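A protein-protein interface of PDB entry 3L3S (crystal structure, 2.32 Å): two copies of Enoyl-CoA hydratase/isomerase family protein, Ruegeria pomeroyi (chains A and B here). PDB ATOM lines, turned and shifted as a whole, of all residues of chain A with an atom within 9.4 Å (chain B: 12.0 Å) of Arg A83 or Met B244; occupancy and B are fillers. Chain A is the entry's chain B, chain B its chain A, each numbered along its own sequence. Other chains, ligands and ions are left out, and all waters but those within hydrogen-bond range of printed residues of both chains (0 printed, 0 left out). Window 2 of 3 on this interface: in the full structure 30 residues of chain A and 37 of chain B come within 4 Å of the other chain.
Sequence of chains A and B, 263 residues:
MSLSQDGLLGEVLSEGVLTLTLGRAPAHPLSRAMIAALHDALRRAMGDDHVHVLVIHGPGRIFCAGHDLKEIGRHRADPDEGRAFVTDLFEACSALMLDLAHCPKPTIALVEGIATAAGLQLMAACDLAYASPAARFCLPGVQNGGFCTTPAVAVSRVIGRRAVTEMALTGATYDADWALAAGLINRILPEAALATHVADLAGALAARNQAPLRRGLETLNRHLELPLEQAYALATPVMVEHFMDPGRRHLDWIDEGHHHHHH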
ATOM      1  N   LYS A  70       7.157 -19.319   2.897  1.00  0.00           N
ATOM      2  CA  LYS A  70       7.015 -18.264   1.891  1.00  0.00           C
ATOM      3  C   LYS A  70       5.848 -17.357   2.294  1.00  0.00           C
ATOM      4  O   LYS A  70       4.929 -17.794   3.008  1.00  0.00           O
ATOM      5  CB  LYS A  70       6.819 -18.843   0.478  1.00  0.00           C
ATOM      6  CG  LYS A  70       5.757 -19.922   0.335  1.00  0.00           C
ATOM      7  CD  LYS A  70       5.476 -20.219  -1.135  1.00  0.00           C
ATOM      8  CE  LYS A  70       4.974 -21.642  -1.345  1.00  0.00           C
ATOM      9  NZ  LYS A  70       4.470 -21.857  -2.724  1.00  0.00           N
ATOM     10  N   GLU A  71       5.865 -16.125   1.778  1.00  0.00           N
ATOM     11  CA  GLU A  71       4.877 -15.108   2.126  1.00  0.00           C
ATOM     12  C   GLU A  71       3.775 -14.670   1.163  1.00  0.00           C
ATOM     13  O   GLU A  71       4.041 -14.048   0.131  1.00  0.00           O
ATOM     14  CB  GLU A  71       5.614 -13.854   2.577  1.00  0.00           C
ATOM     15  CG  GLU A  71       4.841 -13.000   3.572  1.00  0.00           C
ATOM     16  CD  GLU A  71       4.978 -13.509   4.992  1.00  0.00           C
ATOM     17  OE1 GLU A  71       6.044 -14.094   5.318  1.00  0.00           O
ATOM     18  OE2 GLU A  71       4.023 -13.313   5.782  1.00  0.00           O
ATOM     19  N   ILE A  72       2.535 -14.929   1.575  1.00  0.00           N
ATOM     20  CA  ILE A  72       1.334 -14.518   0.850  1.00  0.00           C
ATOM     21  C   ILE A  72       0.551 -13.713   1.896  1.00  0.00           C
ATOM     22  O   ILE A  72       0.154 -14.256   2.929  1.00  0.00           O
ATOM     23  CB  ILE A  72       0.494 -15.733   0.283  1.00  0.00           C
ATOM     24  CG1 ILE A  72       1.207 -16.346  -0.947  1.00  0.00           C
ATOM     25  CG2 ILE A  72      -1.000 -15.295  -0.021  1.00  0.00           C
ATOM     26  CD1 ILE A  72       0.384 -16.489  -2.235  1.00  0.00           C
ATOM     27  N   GLY A  73       0.383 -12.415   1.640  1.00  0.00           N
ATOM     28  CA  GLY A  73      -0.329 -11.548   2.566  1.00  0.00           C
ATOM     29  C   GLY A  73      -1.197 -10.499   1.895  1.00  0.00           C
ATOM     30  O   GLY A  73      -0.732  -9.380   1.652  1.00  0.00           O
ATOM     31  N   ARG A  74      -2.450 -10.866   1.605  1.00  0.00           N
ATOM     32  CA  ARG A  74      -3.424  -9.973   0.969  1.00  0.00           C
ATOM     33  C   ARG A  74      -4.648  -9.727   1.845  1.00  0.00           C
ATOM     34  O   ARG A  74      -4.905  -8.587   2.241  1.00  0.00           O
ATOM     35  CB  ARG A  74      -3.862 -10.520  -0.372  1.00  0.00           C
ATOM     36  N   HIS A  75      -5.416 -10.788   2.112  1.00  0.00           N
ATOM     37  CA  HIS A  75      -6.628 -10.711   2.940  1.00  0.00           C
ATOM     38  C   HIS A  75      -6.339 -10.897   4.432  1.00  0.00           C
ATOM     39  O   HIS A  75      -5.706 -11.879   4.839  1.00  0.00           O
ATOM     40  CB  HIS A  75      -7.694 -11.727   2.459  1.00  0.00           C
ATOM     41  CG  HIS A  75      -7.176 -13.129   2.294  1.00  0.00           C
ATOM     42  ND1 HIS A  75      -6.659 -13.588   1.100  1.00  0.00           N
ATOM     43  CD2 HIS A  75      -7.037 -14.145   3.183  1.00  0.00           C
ATOM     44  CE1 HIS A  75      -6.217 -14.823   1.266  1.00  0.00           C
ATOM     45  NE2 HIS A  75      -6.434 -15.185   2.519  1.00  0.00           N
ATOM     46  N   ARG A  83      -5.071 -16.737   4.395  1.00  0.00           N
ATOM     47  CA  ARG A  83      -5.818 -17.943   4.721  1.00  0.00           C
ATOM     48  C   ARG A  83      -6.000 -18.861   3.525  1.00  0.00           C
ATOM     49  O   ARG A  83      -5.616 -20.023   3.581  1.00  0.00           O
ATOM     50  CB  ARG A  83      -7.202 -17.608   5.299  1.00  0.00           C
ATOM     51  CG  ARG A  83      -7.175 -16.975   6.672  1.00  0.00           C
ATOM     52  CD  ARG A  83      -8.534 -17.028   7.354  1.00  0.00           C
ATOM     53  NE  ARG A  83      -8.389 -17.492   8.733  1.00  0.00           N
ATOM     54  CZ  ARG A  83      -8.627 -18.736   9.138  1.00  0.00           C
ATOM     55  NH1 ARG A  83      -9.047 -19.658   8.278  1.00  0.00           N
ATOM     56  NH2 ARG A  83      -8.376 -19.080  10.393  1.00  0.00           N
ATOM     57  N   ALA A  84      -6.566 -18.323   2.441  1.00  0.00           N
ATOM     58  CA  ALA A  84      -6.850 -19.067   1.204  1.00  0.00           C
ATOM     59  C   ALA A  84      -5.668 -19.845   0.617  1.00  0.00           C
ATOM     60  O   ALA A  84      -5.848 -20.934   0.062  1.00  0.00           O
ATOM     61  CB  ALA A  84      -7.448 -18.136   0.153  1.00  0.00           C
ATOM     62  N   PHE A  85      -4.465 -19.302   0.795  1.00  0.00           N
ATOM     63  CA  PHE A  85      -3.244 -19.937   0.311  1.00  0.00           C
ATOM     64  C   PHE A  85      -2.816 -21.083   1.225  1.00  0.00           C
ATOM     65  O   PHE A  85      -2.384 -22.126   0.737  1.00  0.00           O
ATOM     66  CB  PHE A  85      -2.111 -18.906   0.167  1.00  0.00           C
ATOM     67  CG  PHE A  85      -0.766 -19.513  -0.125  1.00  0.00           C
ATOM     68  CD1 PHE A  85      -0.478 -20.022  -1.404  1.00  0.00           C
ATOM     69  CD2 PHE A  85       0.184 -19.664   0.908  1.00  0.00           C
ATOM     70  CE1 PHE A  85       0.743 -20.691  -1.653  1.00  0.00           C
ATOM     71  CE2 PHE A  85       1.401 -20.327   0.674  1.00  0.00           C
ATOM     72  CZ  PHE A  85       1.678 -20.844  -0.610  1.00  0.00           C
ATOM     73  N   VAL A  86      -2.843 -20.846   2.534  1.00  0.00           N
ATOM     74  CA  VAL A  86      -2.462 -21.864   3.510  1.00  0.00           C
ATOM     75  C   VAL A  86      -3.472 -23.029   3.537  1.00  0.00           C
ATOM     76  O   VAL A  86      -3.083 -24.183   3.704  1.00  0.00           O
ATOM     77  CB  VAL A  86      -2.157 -21.201   4.894  1.00  0.00           C
ATOM     78  CG1 VAL A  86      -2.909 -21.834   6.058  1.00  0.00           C
ATOM     79  CG2 VAL A  86      -0.656 -21.221   5.142  1.00  0.00           C
ATOM     80  N   THR A  87      -4.737 -22.721   3.243  1.00  0.00           N
ATOM     81  CA  THR A  87      -5.818 -23.704   3.191  1.00  0.00           C
ATOM     82  C   THR A  87      -5.654 -24.580   1.943  1.00  0.00           C
ATOM     83  O   THR A  87      -5.857 -25.791   2.004  1.00  0.00           O
ATOM     84  CB  THR A  87      -7.207 -23.007   3.212  1.00  0.00           C
ATOM     85  OG1 THR A  87      -7.327 -22.229   4.413  1.00  0.00           O
ATOM     86  CG2 THR A  87      -8.342 -24.017   3.187  1.00  0.00           C
ATOM     87  N   ASP A  88      -5.231 -23.969   0.838  1.00  0.00           N
ATOM     88  CA  ASP A  88      -4.998 -24.677  -0.422  1.00  0.00           C
ATOM     89  C   ASP A  88      -3.747 -25.558  -0.292  1.00  0.00           C
ATOM     90  O   ASP A  88      -3.744 -26.709  -0.745  1.00  0.00           O
ATOM     91  CB  ASP A  88      -4.841 -23.666  -1.573  1.00  0.00           C
ATOM     92  CG  ASP A  88      -4.403 -24.314  -2.873  1.00  0.00           C
ATOM     93  OD1 ASP A  88      -5.258 -24.879  -3.582  1.00  0.00           O
ATOM     94  OD2 ASP A  88      -3.190 -24.285  -3.163  1.00  0.00           O
ATOM     95  N   LEU A  89      -2.725 -25.009   0.371  1.00  0.00           N
ATOM     96  CA  LEU A  89      -1.438 -25.668   0.602  1.00  0.00           C
ATOM     97  C   LEU A  89      -1.575 -26.964   1.395  1.00  0.00           C
ATOM     98  O   LEU A  89      -1.183 -28.018   0.907  1.00  0.00           O
ATOM     99  CB  LEU A  89      -0.456 -24.709   1.313  1.00  0.00           C
ATOM    100  CG  LEU A  89       0.961 -25.150   1.719  1.00  0.00           C
ATOM    101  CD1 LEU A  89       1.840 -25.391   0.506  1.00  0.00           C
ATOM    102  CD2 LEU A  89       1.588 -24.089   2.603  1.00  0.00           C
ATOM    103  N   PHE A  90      -2.185 -26.872   2.575  1.00  0.00           N
ATOM    104  CA  PHE A  90      -2.381 -28.019   3.456  1.00  0.00           C
ATOM    105  C   PHE A  90      -3.353 -29.091   2.950  1.00  0.00           C
ATOM    106  O   PHE A  90      -3.089 -30.285   3.136  1.00  0.00           O
ATOM    107  CB  PHE A  90      -2.736 -27.558   4.874  1.00  0.00           C
ATOM    108  CG  PHE A  90      -1.664 -26.720   5.532  1.00  0.00           C
ATOM    109  CD1 PHE A  90      -0.296 -27.038   5.389  1.00  0.00           C
ATOM    110  CD2 PHE A  90      -2.014 -25.583   6.274  1.00  0.00           C
ATOM    111  CE1 PHE A  90       0.714 -26.221   5.975  1.00  0.00           C
ATOM    112  CE2 PHE A  90      -1.020 -24.758   6.868  1.00  0.00           C
ATOM    113  CZ  PHE A  90       0.348 -25.080   6.712  1.00  0.00           C
ATOM    114  N   GLU A  91      -4.443 -28.673   2.286  1.00  0.00           N
ATOM    115  CA  GLU A  91      -5.426 -29.611   1.717  1.00  0.00           C
ATOM    116  C   GLU A  91      -4.815 -30.413   0.564  1.00  0.00           C
ATOM    117  O   GLU A  91      -5.114 -31.606   0.394  1.00  0.00           O
ATOM    118  CB  GLU A  91      -6.701 -28.888   1.253  1.00  0.00           C
ATOM    119  CG  GLU A  91      -7.681 -28.562   2.395  1.00  0.00           C
ATOM    120  CD  GLU A  91      -8.803 -27.580   2.024  1.00  0.00           C
ATOM    121  OE1 GLU A  91      -9.556 -27.202   2.946  1.00  0.00           O
ATOM    122  OE2 GLU A  91      -8.941 -27.172   0.845  1.00  0.00           O
ATOM    123  N   GLY A 145       6.244 -21.537  17.268  1.00  0.00           N
ATOM    124  CA  GLY A 145       4.948 -21.021  17.671  1.00  0.00           C
ATOM    125  C   GLY A 145       3.774 -21.704  16.998  1.00  0.00           C
ATOM    126  O   GLY A 145       2.748 -21.069  16.732  1.00  0.00           O
ATOM    127  N   GLY A 146       3.942 -22.999  16.738  1.00  0.00           N
ATOM    128  CA  GLY A 146       2.913 -23.808  16.108  1.00  0.00           C
ATOM    129  C   GLY A 146       2.880 -25.198  16.723  1.00  0.00           C
ATOM    130  O   GLY A 146       3.139 -25.368  17.918  1.00  0.00           O
ATOM    131  N   ASN B 209       4.128 -21.233  22.563  1.00  0.00           N
ATOM    132  CA  ASN B 209       2.819 -20.651  22.229  1.00  0.00           C
ATOM    133  C   ASN B 209       1.726 -21.679  22.549  1.00  0.00           C
ATOM    134  O   ASN B 209       1.630 -22.748  21.936  1.00  0.00           O
ATOM    135  CB  ASN B 209       2.755 -20.189  20.768  1.00  0.00           C
ATOM    136  CG  ASN B 209       1.581 -19.251  20.493  1.00  0.00           C
ATOM    137  OD1 ASN B 209       1.053 -18.609  21.401  1.00  0.00           O
ATOM    138  ND2 ASN B 209       1.163 -19.180  19.236  1.00  0.00           N
ATOM    139  N   GLN B 210       0.962 -21.317  23.574  1.00  0.00           N
ATOM    140  CA  GLN B 210      -0.109 -22.099  24.175  1.00  0.00           C
ATOM    141  C   GLN B 210      -1.352 -22.531  23.390  1.00  0.00           C
ATOM    142  O   GLN B 210      -1.801 -23.678  23.548  1.00  0.00           O
ATOM    143  CB  GLN B 210      -0.511 -21.402  25.478  1.00  0.00           C
ATOM    144  CG  GLN B 210      -0.580 -22.293  26.707  1.00  0.00           C
ATOM    145  CD  GLN B 210       0.596 -23.246  26.883  1.00  0.00           C
ATOM    146  OE1 GLN B 210       0.404 -24.456  26.945  1.00  0.00           O
ATOM    147  NE2 GLN B 210       1.805 -22.706  27.010  1.00  0.00           N
ATOM    148  N   ALA B 211      -1.912 -21.640  22.569  1.00  0.00           N
ATOM    149  CA  ALA B 211      -3.109 -21.985  21.800  1.00  0.00           C
ATOM    150  C   ALA B 211      -2.894 -23.104  20.770  1.00  0.00           C
ATOM    151  O   ALA B 211      -3.614 -24.103  20.821  1.00  0.00           O
ATOM    152  CB  ALA B 211      -3.776 -20.736  21.179  1.00  0.00           C
ATOM    153  N   PRO B 212      -1.852 -23.012  19.900  1.00  0.00           N
ATOM    154  CA  PRO B 212      -1.679 -24.110  18.940  1.00  0.00           C
ATOM    155  C   PRO B 212      -1.174 -25.416  19.570  1.00  0.00           C
ATOM    156  O   PRO B 212      -1.311 -26.477  18.974  1.00  0.00           O
ATOM    157  CB  PRO B 212      -0.675 -23.535  17.940  1.00  0.00           C
ATOM    158  CG  PRO B 212       0.135 -22.611  18.756  1.00  0.00           C
ATOM    159  CD  PRO B 212      -0.920 -21.915  19.567  1.00  0.00           C
ATOM    160  N   LEU B 213      -0.656 -25.331  20.795  1.00  0.00           N
ATOM    161  CA  LEU B 213      -0.140 -26.492  21.524  1.00  0.00           C
ATOM    162  C   LEU B 213      -1.262 -27.392  22.016  1.00  0.00           C
ATOM    163  O   LEU B 213      -1.194 -28.614  21.867  1.00  0.00           O
ATOM    164  CB  LEU B 213       0.718 -26.047  22.720  1.00  0.00           C
ATOM    165  CG  LEU B 213       1.325 -27.098  23.661  1.00  0.00           C
ATOM    166  CD1 LEU B 213       2.356 -27.924  22.924  1.00  0.00           C
ATOM    167  CD2 LEU B 213       1.954 -26.418  24.855  1.00  0.00           C
ATOM    168  N   ARG B 215      -4.528 -27.160  21.007  1.00  0.00           N
ATOM    169  CA  ARG B 215      -5.373 -27.507  19.858  1.00  0.00           C
ATOM    170  C   ARG B 215      -4.755 -28.631  19.043  1.00  0.00           C
ATOM    171  O   ARG B 215      -5.471 -29.414  18.426  1.00  0.00           O
ATOM    172  CB  ARG B 215      -5.619 -26.292  18.954  1.00  0.00           C
ATOM    173  CG  ARG B 215      -6.773 -25.392  19.396  1.00  0.00           C
ATOM    174  CD  ARG B 215      -8.144 -26.051  19.194  1.00  0.00           C
ATOM    175  NE  ARG B 215      -8.514 -26.190  17.785  1.00  0.00           N
ATOM    176  CZ  ARG B 215      -9.283 -27.165  17.295  1.00  0.00           C
ATOM    177  NH1 ARG B 215      -9.768 -28.111  18.093  1.00  0.00           N
ATOM    178  NH2 ARG B 215      -9.611 -27.169  16.006  1.00  0.00           N
ATOM    179  N   ALA B 235      -7.500 -32.960  11.007  1.00  0.00           N
ATOM    180  CA  ALA B 235      -6.203 -32.308  11.197  1.00  0.00           C
ATOM    181  C   ALA B 235      -5.849 -31.132  10.288  1.00  0.00           C
ATOM    182  O   ALA B 235      -5.206 -30.193  10.741  1.00  0.00           O
ATOM    183  CB  ALA B 235      -5.094 -33.342  11.179  1.00  0.00           C
ATOM    184  N   THR B 236      -6.273 -31.174   9.026  1.00  0.00           N
ATOM    185  CA  THR B 236      -5.990 -30.093   8.074  1.00  0.00           C
ATOM    186  C   THR B 236      -6.531 -28.700   8.491  1.00  0.00           C
ATOM    187  O   THR B 236      -5.745 -27.749   8.492  1.00  0.00           O
ATOM    188  CB  THR B 236      -6.362 -30.482   6.612  1.00  0.00           C
ATOM    189  OG1 THR B 236      -5.737 -31.722   6.274  1.00  0.00           O
ATOM    190  CG2 THR B 236      -5.882 -29.439   5.653  1.00  0.00           C
ATOM    191  N   PRO B 237      -7.835 -28.558   8.882  1.00  0.00           N
ATOM    192  CA  PRO B 237      -8.258 -27.201   9.277  1.00  0.00           C
ATOM    193  C   PRO B 237      -7.581 -26.703  10.571  1.00  0.00           C
ATOM    194  O   PRO B 237      -7.433 -25.495  10.768  1.00  0.00           O
ATOM    195  CB  PRO B 237      -9.781 -27.338   9.437  1.00  0.00           C
ATOM    196  CG  PRO B 237      -9.973 -28.762   9.784  1.00  0.00           C
ATOM    197  CD  PRO B 237      -9.023 -29.438   8.830  1.00  0.00           C
ATOM    198  N   VAL B 238      -7.137 -27.646  11.405  1.00  0.00           N
ATOM    199  CA  VAL B 238      -6.439 -27.349  12.664  1.00  0.00           C
ATOM    200  C   VAL B 238      -5.023 -26.847  12.331  1.00  0.00           C
ATOM    201  O   VAL B 238      -4.518 -25.940  12.986  1.00  0.00           O
ATOM    202  CB  VAL B 238      -6.363 -28.603  13.603  1.00  0.00           C
ATOM    203  CG1 VAL B 238      -5.604 -28.285  14.897  1.00  0.00           C
ATOM    204  CG2 VAL B 238      -7.755 -29.102  13.943  1.00  0.00           C
ATOM    205  N   MET B 239      -4.423 -27.416  11.281  1.00  0.00           N
ATOM    206  CA  MET B 239      -3.091 -27.028  10.820  1.00  0.00           C
ATOM    207  C   MET B 239      -3.156 -25.627  10.192  1.00  0.00           C
ATOM    208  O   MET B 239      -2.185 -24.876  10.249  1.00  0.00           O
ATOM    209  CB  MET B 239      -2.554 -28.063   9.833  1.00  0.00           C
ATOM    210  CG  MET B 239      -1.169 -27.785   9.248  1.00  0.00           C
ATOM    211  SD  MET B 239       0.286 -27.996  10.488  1.00  0.00           S
ATOM    212  CE  MET B 239       1.742 -28.290   9.243  1.00  0.00           C
ATOM    213  N   VAL B 240      -4.320 -25.276   9.639  1.00  0.00           N
ATOM    214  CA  VAL B 240      -4.550 -23.956   9.045  1.00  0.00           C
ATOM    215  C   VAL B 240      -4.639 -22.933  10.180  1.00  0.00           C
ATOM    216  O   VAL B 240      -4.020 -21.866  10.119  1.00  0.00           O
ATOM    217  CB  VAL B 240      -5.845 -23.952   8.183  1.00  0.00           C
ATOM    218  CG1 VAL B 240      -6.280 -22.522   7.771  1.00  0.00           C
ATOM    219  CG2 VAL B 240      -5.621 -24.797   6.953  1.00  0.00           C
ATOM    220  N   GLU B 241      -5.325 -23.333  11.250  1.00  0.00           N
ATOM    221  CA  GLU B 241      -5.520 -22.512  12.442  1.00  0.00           C
ATOM    222  C   GLU B 241      -4.202 -22.209  13.169  1.00  0.00           C
ATOM    223  O   GLU B 241      -4.070 -21.138  13.763  1.00  0.00           O
ATOM    224  CB  GLU B 241      -6.522 -23.204  13.380  1.00  0.00           C
ATOM    225  CG  GLU B 241      -7.025 -22.360  14.555  1.00  0.00           C
ATOM    226  CD  GLU B 241      -8.099 -23.061  15.383  1.00  0.00           C
ATOM    227  OE1 GLU B 241      -8.059 -24.309  15.504  1.00  0.00           O
ATOM    228  OE2 GLU B 241      -8.986 -22.351  15.915  1.00  0.00           O
ATOM    229  N   HIS B 242      -3.224 -23.120  13.076  1.00  0.00           N
ATOM    230  CA  HIS B 242      -1.908 -22.950  13.721  1.00  0.00           C
ATOM    231  C   HIS B 242      -1.152 -21.791  13.104  1.00  0.00           C
ATOM    232  O   HIS B 242      -0.694 -20.901  13.811  1.00  0.00           O
ATOM    233  CB  HIS B 242      -1.028 -24.197  13.576  1.00  0.00           C
ATOM    234  CG  HIS B 242      -1.481 -25.374  14.378  1.00  0.00           C
ATOM    235  ND1 HIS B 242      -2.211 -25.260  15.540  1.00  0.00           N
ATOM    236  CD2 HIS B 242      -1.294 -26.700  14.181  1.00  0.00           C
ATOM    237  CE1 HIS B 242      -2.456 -26.466  16.021  1.00  0.00           C
ATOM    238  NE2 HIS B 242      -1.910 -27.355  15.216  1.00  0.00           N
ATOM    239  N   PHE B 243      -1.103 -21.798  11.771  1.00  0.00           N
ATOM    240  CA  PHE B 243      -0.428 -20.786  10.962  1.00  0.00           C
ATOM    241  C   PHE B 243      -1.096 -19.420  10.985  1.00  0.00           C
ATOM    242  O   PHE B 243      -0.520 -18.437  10.531  1.00  0.00           O
ATOM    243  CB  PHE B 243      -0.266 -21.293   9.523  1.00  0.00           C
ATOM    244  CG  PHE B 243       0.913 -22.203   9.343  1.00  0.00           C
ATOM    245  CD1 PHE B 243       2.051 -21.757   8.648  1.00  0.00           C
ATOM    246  CD2 PHE B 243       0.922 -23.492   9.919  1.00  0.00           C
ATOM    247  CE1 PHE B 243       3.201 -22.578   8.527  1.00  0.00           C
ATOM    248  CE2 PHE B 243       2.062 -24.333   9.814  1.00  0.00           C
ATOM    249  CZ  PHE B 243       3.210 -23.874   9.114  1.00  0.00           C
ATOM    250  N   MET B 244      -2.316 -19.377  11.514  1.00  0.00           N
ATOM    251  CA  MET B 244      -3.082 -18.140  11.635  1.00  0.00           C
ATOM    252  C   MET B 244      -3.223 -17.816  13.139  1.00  0.00           C
ATOM    253  O   MET B 244      -3.829 -16.779  13.485  1.00  0.00           O
ATOM    254  CB  MET B 244      -4.465 -18.283  10.954  1.00  0.00           C
ATOM    255  CG  MET B 244      -4.454 -18.649   9.452  1.00  0.00           C
ATOM    256  SD  MET B 244      -3.791 -17.315   8.153  1.00  0.00           S
ATOM    257  CE  MET B 244      -2.195 -18.224   7.525  1.00  0.00           C
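A ring nitrogen (NE2) of His A75 lies within hydrogen-bond range of the backbone NH (N) of Arg A83, at 2.8 Å.
O of Arg A83 lies within hydrogen-bond range of OG1 of Thr A87 (2.9 Å).
Arg A83 touches Met B244 (CG to SD, 3.7 Å).
CG1 of Val A86 touches CG1 of Val B240, 3.8 Å away.
Val A86 touches Met B244 (CG1 to CE, 3.96 Å).
OG1 of Thr A87 touches CG1 of Val B240, at 3.5 Å.
Phe A90 touches Thr B236 (C to CG2, 3.7 Å).
Val B240 touches Phe A90 (CG2 to CD2, 3.8 Å).
Phe A90 touches Phe B243 (CZ to CE2, 3.6 Å).
Glu A91 touches Thr B236.
Asn B209 touches Gly A145.
Gly A145 touches Pro B212.
Printed residues of chain B within 4 Å of Arg A83: Met B244 (3.7 Å).
Met B244 touches just these residues of chain A: Arg A83 (3.7 Å) and Val A86 (3.96 Å).
His A75 touches none of the printed residues of chain B.
No residue of chain B comes within 4 Å of Ala A84.
Val A86 touches two residues of chain B.
Of chain B, only Val B240 comes within 4 Å of Thr A87.
Of the printed residues of chain A, Phe B243 touches Phe A90.
Of the printed residues of chain A, Val B240 touches Val A86, Thr A87 and Phe A90.
Of the printed residues of chain A, Asn B209 touches Gly A145.
Of the printed residues of chain B, Gly A145 touches Asn B209 (3.5 Å) and Pro B212 (3.6 Å).
Printed residues of chain B within 4 Å of Phe A90: Thr B236, Met B239, Val B240 and Phe B243.
Gln B210 touches none of the printed residues of chain A.
The nearest printed residue of chain A that does not touch Thr B236 is Thr A87 (5.2 Å).
Of the 17 printed residues of chain A, 6 touch a printed residue of chain B.
Hydrophobic or aromatic side chains of chain B within 4 Å of the printed part of chain A: Pro B212, Met B239, Val B240, Phe B243 and Met B244.
No position is printed for both chains.
Of the 11 pairs that touch across the chains among the printed residues, none has its exchanged pair printed and touching as well.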
